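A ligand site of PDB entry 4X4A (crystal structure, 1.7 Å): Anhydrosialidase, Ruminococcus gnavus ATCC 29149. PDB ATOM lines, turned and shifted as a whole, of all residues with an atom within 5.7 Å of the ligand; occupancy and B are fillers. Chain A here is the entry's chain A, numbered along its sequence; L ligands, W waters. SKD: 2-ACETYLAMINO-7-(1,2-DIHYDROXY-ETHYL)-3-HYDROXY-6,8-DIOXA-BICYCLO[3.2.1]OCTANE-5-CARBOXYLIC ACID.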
ATOM      1  N   ARG A  23      22.161  -4.091 -17.052  1.00  0.00           N
ATOM      2  CA  ARG A  23      21.390  -3.699 -18.268  1.00  0.00           C
ATOM      3  C   ARG A  23      22.408  -3.042 -19.181  1.00  0.00           C
ATOM      4  O   ARG A  23      23.489  -2.694 -18.763  1.00  0.00           O
ATOM      5  CB  ARG A  23      20.272  -2.729 -17.926  1.00  0.00           C
ATOM      6  CG  ARG A  23      18.944  -3.382 -17.597  1.00  0.00           C
ATOM      7  CD  ARG A  23      17.781  -2.423 -17.865  1.00  0.00           C
ATOM      8  NE  ARG A  23      17.695  -2.128 -19.313  1.00  0.00           N
ATOM      9  CZ  ARG A  23      16.970  -1.182 -19.895  1.00  0.00           C
ATOM     10  NH1 ARG A  23      16.179  -0.378 -19.197  1.00  0.00           N
ATOM     11  NH2 ARG A  23      17.100  -0.997 -21.247  1.00  0.00           N
ATOM     12  N   ILE A  24      22.018  -2.806 -20.442  1.00  0.00           N
ATOM     13  CA  ILE A  24      22.720  -1.900 -21.364  1.00  0.00           C
ATOM     14  C   ILE A  24      24.025  -2.485 -21.892  1.00  0.00           C
ATOM     15  O   ILE A  24      25.132  -2.000 -21.525  1.00  0.00           O
ATOM     16  CB  ILE A  24      22.903  -0.460 -20.864  1.00  0.00           C
ATOM     17  CG1 ILE A  24      21.797   0.106 -19.969  1.00  0.00           C
ATOM     18  CG2 ILE A  24      23.063   0.439 -22.093  1.00  0.00           C
ATOM     19  CD1 ILE A  24      20.400   0.095 -20.561  1.00  0.00           C
ATOM     20  N   ASP A  40      25.900  -1.563 -17.661  1.00  0.00           N
ATOM     21  CA  ASP A  40      25.570  -1.042 -16.387  1.00  0.00           C
ATOM     22  C   ASP A  40      25.518  -2.104 -15.356  1.00  0.00           C
ATOM     23  O   ASP A  40      24.779  -3.111 -15.517  1.00  0.00           O
ATOM     24  CB  ASP A  40      24.145  -0.402 -16.330  1.00  0.00           C
ATOM     25  CG  ASP A  40      23.972   0.867 -17.035  1.00  0.00           C
ATOM     26  OD1 ASP A  40      24.834   1.472 -17.732  1.00  0.00           O
ATOM     27  OD2 ASP A  40      22.801   1.351 -16.905  1.00  0.00           O
ATOM     28  N   ARG A  42      23.681  -2.273 -12.260  1.00  0.00           N
ATOM     29  CA  ARG A  42      22.551  -1.589 -11.620  1.00  0.00           C
ATOM     30  C   ARG A  42      22.306  -2.274 -10.237  1.00  0.00           C
ATOM     31  O   ARG A  42      21.680  -3.350 -10.127  1.00  0.00           O
ATOM     32  CB  ARG A  42      21.301  -1.582 -12.516  1.00  0.00           C
ATOM     33  CG  ARG A  42      21.534  -0.948 -13.884  1.00  0.00           C
ATOM     34  CD  ARG A  42      20.262  -0.602 -14.572  1.00  0.00           C
ATOM     35  NE  ARG A  42      20.511   0.299 -15.693  1.00  0.00           N
ATOM     36  CZ  ARG A  42      19.580   0.927 -16.402  1.00  0.00           C
ATOM     37  NH1 ARG A  42      18.335   0.785 -16.120  1.00  0.00           N
ATOM     38  NH2 ARG A  42      19.968   1.765 -17.408  1.00  0.00           N
ATOM     39  N   ASP A  48      16.663   2.835 -14.096  1.00  0.00           N
ATOM     40  CA  ASP A  48      17.573   3.830 -14.647  1.00  0.00           C
ATOM     41  C   ASP A  48      17.972   4.791 -13.507  1.00  0.00           C
ATOM     42  O   ASP A  48      17.316   4.817 -12.455  1.00  0.00           O
ATOM     43  CB  ASP A  48      16.867   4.694 -15.672  1.00  0.00           C
ATOM     44  CG  ASP A  48      16.138   3.918 -16.735  1.00  0.00           C
ATOM     45  OD1 ASP A  48      16.559   2.778 -17.162  1.00  0.00           O
ATOM     46  OD2 ASP A  48      15.125   4.507 -17.198  1.00  0.00           O
ATOM     47  N   ALA A  49      18.964   5.620 -13.757  1.00  0.00           N
ATOM     48  CA  ALA A  49      19.311   6.660 -12.846  1.00  0.00           C
ATOM     49  C   ALA A  49      18.061   7.595 -12.798  1.00  0.00           C
ATOM     50  O   ALA A  49      17.425   7.776 -13.820  1.00  0.00           O
ATOM     51  CB  ALA A  49      20.534   7.393 -13.327  1.00  0.00           C
ATOM     52  N   ILE A 104      25.877   5.582 -16.251  1.00  0.00           N
ATOM     53  CA  ILE A 104      24.837   4.861 -16.919  1.00  0.00           C
ATOM     54  C   ILE A 104      25.038   4.958 -18.408  1.00  0.00           C
ATOM     55  O   ILE A 104      25.425   6.054 -18.900  1.00  0.00           O
ATOM     56  CB  ILE A 104      23.453   5.409 -16.520  1.00  0.00           C
ATOM     57  CG1 ILE A 104      22.346   4.718 -17.321  1.00  0.00           C
ATOM     58  CG2 ILE A 104      23.329   6.954 -16.589  1.00  0.00           C
ATOM     59  CD1 ILE A 104      20.951   4.893 -16.699  1.00  0.00           C
ATOM     60  N   ASP A 105      24.733   3.831 -19.108  1.00  0.00           N
ATOM     61  CA  ASP A 105      24.622   3.744 -20.534  1.00  0.00           C
ATOM     62  C   ASP A 105      26.023   3.817 -21.240  1.00  0.00           C
ATOM     63  O   ASP A 105      26.377   4.811 -21.894  1.00  0.00           O
ATOM     64  CB  ASP A 105      23.685   4.817 -21.174  1.00  0.00           C
ATOM     65  CG  ASP A 105      22.208   4.497 -20.971  1.00  0.00           C
ATOM     66  OD1 ASP A 105      21.848   3.407 -20.391  1.00  0.00           O
ATOM     67  OD2 ASP A 105      21.372   5.381 -21.433  1.00  0.00           O
ATOM     68  N   ASP A 122      27.254   8.063 -19.438  1.00  0.00           N
ATOM     69  CA  ASP A 122      26.602   9.205 -18.807  1.00  0.00           C
ATOM     70  C   ASP A 122      27.046   9.275 -17.336  1.00  0.00           C
ATOM     71  O   ASP A 122      27.005   8.275 -16.664  1.00  0.00           O
ATOM     72  CB  ASP A 122      25.073   9.184 -18.874  1.00  0.00           C
ATOM     73  CG  ASP A 122      24.537   8.933 -20.253  1.00  0.00           C
ATOM     74  OD1 ASP A 122      25.152   9.330 -21.299  1.00  0.00           O
ATOM     75  OD2 ASP A 122      23.434   8.329 -20.311  1.00  0.00           O
ATOM     76  N   MET A 124      26.009  11.030 -13.809  1.00  0.00           N
ATOM     77  CA  MET A 124      24.879  11.628 -13.155  1.00  0.00           C
ATOM     78  C   MET A 124      25.219  12.011 -11.715  1.00  0.00           C
ATOM     79  O   MET A 124      25.613  11.168 -10.930  1.00  0.00           O
ATOM     80  CB  MET A 124      23.684  10.693 -13.113  1.00  0.00           C
ATOM     81  CG  MET A 124      23.252  10.114 -14.469  1.00  0.00           C
ATOM     82  SD  MET A 124      22.565  11.381 -15.487  1.00  0.00           S
ATOM     83  CE  MET A 124      21.934  10.339 -16.813  1.00  0.00           C
ATOM     84  N   SER A 130      18.255  11.366 -16.328  1.00  0.00           N
ATOM     85  CA  SER A 130      17.924  12.186 -17.444  1.00  0.00           C
ATOM     86  C   SER A 130      16.580  12.887 -17.169  1.00  0.00           C
ATOM     87  O   SER A 130      16.403  14.028 -17.574  1.00  0.00           O
ATOM     88  CB  SER A 130      18.052  11.413 -18.799  1.00  0.00           C
ATOM     89  OG  SER A 130      17.116  10.341 -18.786  1.00  0.00           O
ATOM     90  N   VAL A 268      23.066  12.855 -23.647  1.00  0.00           N
ATOM     91  CA  VAL A 268      23.508  11.544 -23.210  1.00  0.00           C
ATOM     92  C   VAL A 268      23.899  10.684 -24.425  1.00  0.00           C
ATOM     93  O   VAL A 268      23.608  11.037 -25.595  1.00  0.00           O
ATOM     94  CB  VAL A 268      22.376  10.898 -22.372  1.00  0.00           C
ATOM     95  CG1 VAL A 268      22.156  11.657 -21.064  1.00  0.00           C
ATOM     96  CG2 VAL A 268      21.080  10.781 -23.155  1.00  0.00           C
ATOM     97  N   TYR A 291      22.115  11.663 -27.822  1.00  0.00           N
ATOM     98  CA  TYR A 291      20.796  12.275 -28.001  1.00  0.00           C
ATOM     99  C   TYR A 291      20.482  13.215 -26.871  1.00  0.00           C
ATOM    100  O   TYR A 291      21.077  13.158 -25.820  1.00  0.00           O
ATOM    101  CB  TYR A 291      19.668  11.213 -28.205  1.00  0.00           C
ATOM    102  CG  TYR A 291      19.367  10.423 -26.951  1.00  0.00           C
ATOM    103  CD1 TYR A 291      20.077   9.266 -26.660  1.00  0.00           C
ATOM    104  CD2 TYR A 291      18.329  10.798 -26.066  1.00  0.00           C
ATOM    105  CE1 TYR A 291      19.815   8.528 -25.535  1.00  0.00           C
ATOM    106  CE2 TYR A 291      18.032  10.048 -24.946  1.00  0.00           C
ATOM    107  CZ  TYR A 291      18.790   8.920 -24.643  1.00  0.00           C
ATOM    108  OH  TYR A 291      18.575   8.159 -23.513  1.00  0.00           O
ATOM    109  N   THR A 323      13.917   9.222 -26.815  1.00  0.00           N
ATOM    110  CA  THR A 323      15.138   8.421 -26.553  1.00  0.00           C
ATOM    111  C   THR A 323      15.718   7.954 -27.885  1.00  0.00           C
ATOM    112  O   THR A 323      15.610   6.793 -28.257  1.00  0.00           O
ATOM    113  CB  THR A 323      14.772   7.271 -25.575  1.00  0.00           C
ATOM    114  OG1 THR A 323      14.102   7.812 -24.436  1.00  0.00           O
ATOM    115  CG2 THR A 323      15.976   6.508 -25.140  1.00  0.00           C
ATOM    116  N   GLU A 325      18.330   6.866 -29.309  1.00  0.00           N
ATOM    117  CA  GLU A 325      19.551   6.050 -29.299  1.00  0.00           C
ATOM    118  C   GLU A 325      19.887   5.570 -30.687  1.00  0.00           C
ATOM    119  O   GLU A 325      19.078   4.931 -31.331  1.00  0.00           O
ATOM    120  CB  GLU A 325      19.346   4.871 -28.383  1.00  0.00           C
ATOM    121  CG  GLU A 325      19.075   5.242 -26.897  1.00  0.00           C
ATOM    122  CD  GLU A 325      18.397   4.128 -26.151  1.00  0.00           C
ATOM    123  OE1 GLU A 325      17.673   3.372 -26.810  1.00  0.00           O
ATOM    124  OE2 GLU A 325      18.622   3.990 -24.891  1.00  0.00           O
ATOM    125  N   ARG A 341      16.619   4.596 -32.819  1.00  0.00           N
ATOM    126  CA  ARG A 341      15.375   4.586 -32.169  1.00  0.00           C
ATOM    127  C   ARG A 341      14.742   5.981 -32.261  1.00  0.00           C
ATOM    128  O   ARG A 341      15.449   6.991 -32.319  1.00  0.00           O
ATOM    129  CB  ARG A 341      15.632   4.215 -30.711  1.00  0.00           C
ATOM    130  CG  ARG A 341      14.466   4.268 -29.762  1.00  0.00           C
ATOM    131  CD  ARG A 341      14.862   3.807 -28.369  1.00  0.00           C
ATOM    132  NE  ARG A 341      13.796   3.983 -27.369  1.00  0.00           N
ATOM    133  CZ  ARG A 341      13.903   3.701 -26.066  1.00  0.00           C
ATOM    134  NH1 ARG A 341      15.062   3.210 -25.638  1.00  0.00           N
ATOM    135  NH2 ARG A 341      12.874   3.927 -25.205  1.00  0.00           N
ATOM    136  N   GLY A 374       9.961   2.746 -28.499  1.00  0.00           N
ATOM    137  CA  GLY A 374      11.146   2.240 -29.186  1.00  0.00           C
ATOM    138  C   GLY A 374      12.088   1.478 -28.229  1.00  0.00           C
ATOM    139  O   GLY A 374      11.850   1.417 -27.010  1.00  0.00           O
ATOM    140  N   ARG A 403       8.772  -5.501 -25.812  1.00  0.00           N
ATOM    141  CA  ARG A 403      10.093  -5.761 -26.287  1.00  0.00           C
ATOM    142  C   ARG A 403      10.327  -7.279 -26.326  1.00  0.00           C
ATOM    143  O   ARG A 403      10.621  -7.907 -25.285  1.00  0.00           O
ATOM    144  CB  ARG A 403      11.134  -5.068 -25.386  1.00  0.00           C
ATOM    145  CG  ARG A 403      11.136  -3.548 -25.411  1.00  0.00           C
ATOM    146  CD  ARG A 403      12.233  -2.892 -24.556  1.00  0.00           C
ATOM    147  NE  ARG A 403      12.334  -1.472 -24.832  1.00  0.00           N
ATOM    148  CZ  ARG A 403      12.922  -0.560 -24.070  1.00  0.00           C
ATOM    149  NH1 ARG A 403      13.527  -0.899 -22.904  1.00  0.00           N
ATOM    150  NH2 ARG A 403      12.997   0.651 -24.514  1.00  0.00           N
ATOM    151  N   TYR A 443      17.638  -4.509 -25.112  1.00  0.00           N
ATOM    152  CA  TYR A 443      18.840  -3.880 -25.635  1.00  0.00           C
ATOM    153  C   TYR A 443      19.814  -4.958 -26.073  1.00  0.00           C
ATOM    154  O   TYR A 443      19.806  -6.078 -25.531  1.00  0.00           O
ATOM    155  CB  TYR A 443      19.479  -2.933 -24.639  1.00  0.00           C
ATOM    156  CG  TYR A 443      18.824  -1.575 -24.423  1.00  0.00           C
ATOM    157  CD1 TYR A 443      17.439  -1.355 -24.522  1.00  0.00           C
ATOM    158  CD2 TYR A 443      19.617  -0.443 -24.175  1.00  0.00           C
ATOM    159  CE1 TYR A 443      16.885  -0.076 -24.326  1.00  0.00           C
ATOM    160  CE2 TYR A 443      19.075   0.802 -23.979  1.00  0.00           C
ATOM    161  CZ  TYR A 443      17.695   0.979 -24.087  1.00  0.00           C
ATOM    162  OH  TYR A 443      17.166   2.199 -23.820  1.00  0.00           O
ATOM    163  N   SER A 463      12.757  -5.037 -20.884  1.00  0.00           N
ATOM    164  CA  SER A 463      13.293  -4.091 -19.903  1.00  0.00           C
ATOM    165  C   SER A 463      12.511  -2.797 -19.827  1.00  0.00           C
ATOM    166  O   SER A 463      12.878  -1.895 -19.054  1.00  0.00           O
ATOM    167  CB  SER A 463      14.773  -3.796 -20.257  1.00  0.00           C
ATOM    168  OG  SER A 463      14.834  -3.198 -21.559  1.00  0.00           O
ATOM    169  N   TRP A 464      11.428  -2.670 -20.602  1.00  0.00           N
ATOM    170  CA  TRP A 464      10.527  -1.526 -20.441  1.00  0.00           C
ATOM    171  C   TRP A 464       9.451  -1.859 -19.434  1.00  0.00           C
ATOM    172  O   TRP A 464       9.040  -1.015 -18.660  1.00  0.00           O
ATOM    173  CB  TRP A 464       9.922  -1.165 -21.779  1.00  0.00           C
ATOM    174  CG  TRP A 464       9.043  -0.007 -21.744  1.00  0.00           C
ATOM    175  CD1 TRP A 464       7.644   0.017 -21.629  1.00  0.00           C
ATOM    176  CD2 TRP A 464       9.445   1.359 -21.888  1.00  0.00           C
ATOM    177  NE1 TRP A 464       7.200   1.310 -21.702  1.00  0.00           N
ATOM    178  CE2 TRP A 464       8.277   2.146 -21.904  1.00  0.00           C
ATOM    179  CE3 TRP A 464      10.684   1.990 -22.052  1.00  0.00           C
ATOM    180  CZ2 TRP A 464       8.327   3.514 -22.029  1.00  0.00           C
ATOM    181  CZ3 TRP A 464      10.709   3.345 -22.213  1.00  0.00           C
ATOM    182  CH2 TRP A 464       9.528   4.096 -22.206  1.00  0.00           C
HETATM  183  C1  SKD L   1      15.026   2.270 -22.028  1.00  0.00           C
HETATM  184  C2  SKD L   1      15.881   3.253 -21.296  1.00  0.00           C
HETATM  185  C3  SKD L   1      17.090   2.642 -20.596  1.00  0.00           C
HETATM  186  C4  SKD L   1      18.262   3.611 -20.616  1.00  0.00           C
HETATM  187  C5  SKD L   1      17.694   4.985 -20.281  1.00  0.00           C
HETATM  188  C6  SKD L   1      16.490   5.363 -21.162  1.00  0.00           C
HETATM  189  C7  SKD L   1      15.187   5.262 -20.408  1.00  0.00           C
HETATM  190  C8  SKD L   1      14.034   5.899 -21.249  1.00  0.00           C
HETATM  191  C9  SKD L   1      12.702   6.028 -20.532  1.00  0.00           C
HETATM  192  C10 SKD L   1      18.806   7.043 -19.427  1.00  0.00           C
HETATM  193  C11 SKD L   1      19.997   7.939 -19.577  1.00  0.00           C
HETATM  194  N5  SKD L   1      18.710   6.061 -20.285  1.00  0.00           N
HETATM  195  O1A SKD L   1      14.267   2.703 -22.923  1.00  0.00           O
HETATM  196  O1B SKD L   1      15.009   1.103 -21.593  1.00  0.00           O
HETATM  197  O4  SKD L   1      19.294   3.270 -19.592  1.00  0.00           O
HETATM  198  O6  SKD L   1      16.352   4.322 -22.123  1.00  0.00           O
HETATM  199  O7  SKD L   1      15.037   3.866 -20.298  1.00  0.00           O
HETATM  200  O8  SKD L   1      14.504   7.202 -21.622  1.00  0.00           O
HETATM  201  O9  SKD L   1      12.622   4.989 -19.570  1.00  0.00           O
HETATM  202  O10 SKD L   1      17.972   7.189 -18.538  1.00  0.00           O
HETATM  203  O   HOH W   1      18.662   8.419 -16.199  1.00  0.00           O
HETATM  204  O   HOH W   2      17.325   9.402 -21.317  1.00  0.00           O
HETATM  205  O   HOH W   3      19.729   5.835 -23.470  1.00  0.00           O
HETATM  206  O   HOH W   4      15.647   8.027 -17.748  1.00  0.00           O
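An oxygen (O4) of the ligand sits at hydrogen-bond distance from the side-chain carboxylate (OD1) of Asp 105, 2.7 Å away.
An oxygen (O1A) of the ligand lies within salt-bridge range of the guanidinium group (NH1) of Arg 341 (2.9 Å).
An oxygen (O1B) of the ligand lies within salt-bridge range of the guanidinium group (NH2) of Arg 23 (3.0 Å).
An oxygen (O4) of the ligand lies within hydrogen-bond range of the guanidinium group (NH2) of Arg 42 (2.7 Å).
An oxygen (O10) of the ligand sits at hydrogen-bond distance from the side-chain hydroxyl of Ser 130, 3.3 Å away.
OD2 of Asp 48 sits close to O9 of the ligand (3.5 Å).
The side-chain hydroxyl (OH) of Tyr 443 lies close to an oxygen (O6) of the ligand (2.8 Å).
The side-chain hydroxyl of Thr 323 is in hydrogen-bond range of an oxygen (O8) of the ligand, at 2.9 Å.
An oxygen (O1B) of the ligand lies within salt-bridge range of the guanidinium group of Arg 403 (2.8 Å).
The backbone NH (N) of Asp 105 sits at hydrogen-bond distance from the side-chain carboxylate (OD1) of Asp 40.
The backbone carbonyl oxygen (O) of Val 268 lies within hydrogen-bond range of the backbone NH (N) of Tyr 291, at 2.8 Å.
OD1 of Asp 105 is in salt-bridge range of NH2 of Arg 42, at 3.9 Å.
OD1 of Asp 48 lies within salt-bridge range of NH1 of Arg 23.
The guanidinium group (NH1) of Arg 341 is in salt-bridge range of the side-chain carboxylate (OE1) of Glu 325 (2.9 Å).
The backbone carbonyl oxygen (O) of Gly 374 sits close to the guanidinium group (NE) of Arg 341 (3.2 Å).
The side-chain hydroxyl (OG) of Ser 463 lies within hydrogen-bond range of the guanidinium group (NH2) of Arg 23 (3.2 Å).
The guanidinium group (NH1) of Arg 341 is in hydrogen-bond range of the side-chain hydroxyl (OH) of Tyr 443, at 3.0 Å.
CD1 of Ile 24 touches O4 of the ligand, 3.5 Å away.
Ile 104 touches the ligand (CD1 to O4, 3.7 Å).
Asp 122 touches the ligand.
Tyr 291 touches the ligand (OH to N5, 3.9 Å).
Glu 325 touches the ligand (OE2 to O6, 3.6 Å).
CZ3 of Trp 464 touches O9 of the ligand, 3.7 Å away.
Hydrophobic or aromatic side chains that line the ligand: Ile 24, Ile 104, Tyr 443 and Trp 464.
Water W4 lies within hydrogen-bond range of an oxygen (O10) of the ligand and the side-chain hydroxyl of Ser 130.
Water W1 lies within hydrogen-bond range of O10 of the ligand (2.7 Å), O of Ala 49 (2.8 Å) and N of Ser 130 (3.0 Å).
Water W3 lies within hydrogen-bond range of OE2 of Glu 325, OH of Tyr 291, OD2 of Asp 105 and N5 of the ligand.
Water W2 bridges OG of Ser 130 (2.7 Å) and OH of Tyr 291 (2.8 Å).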
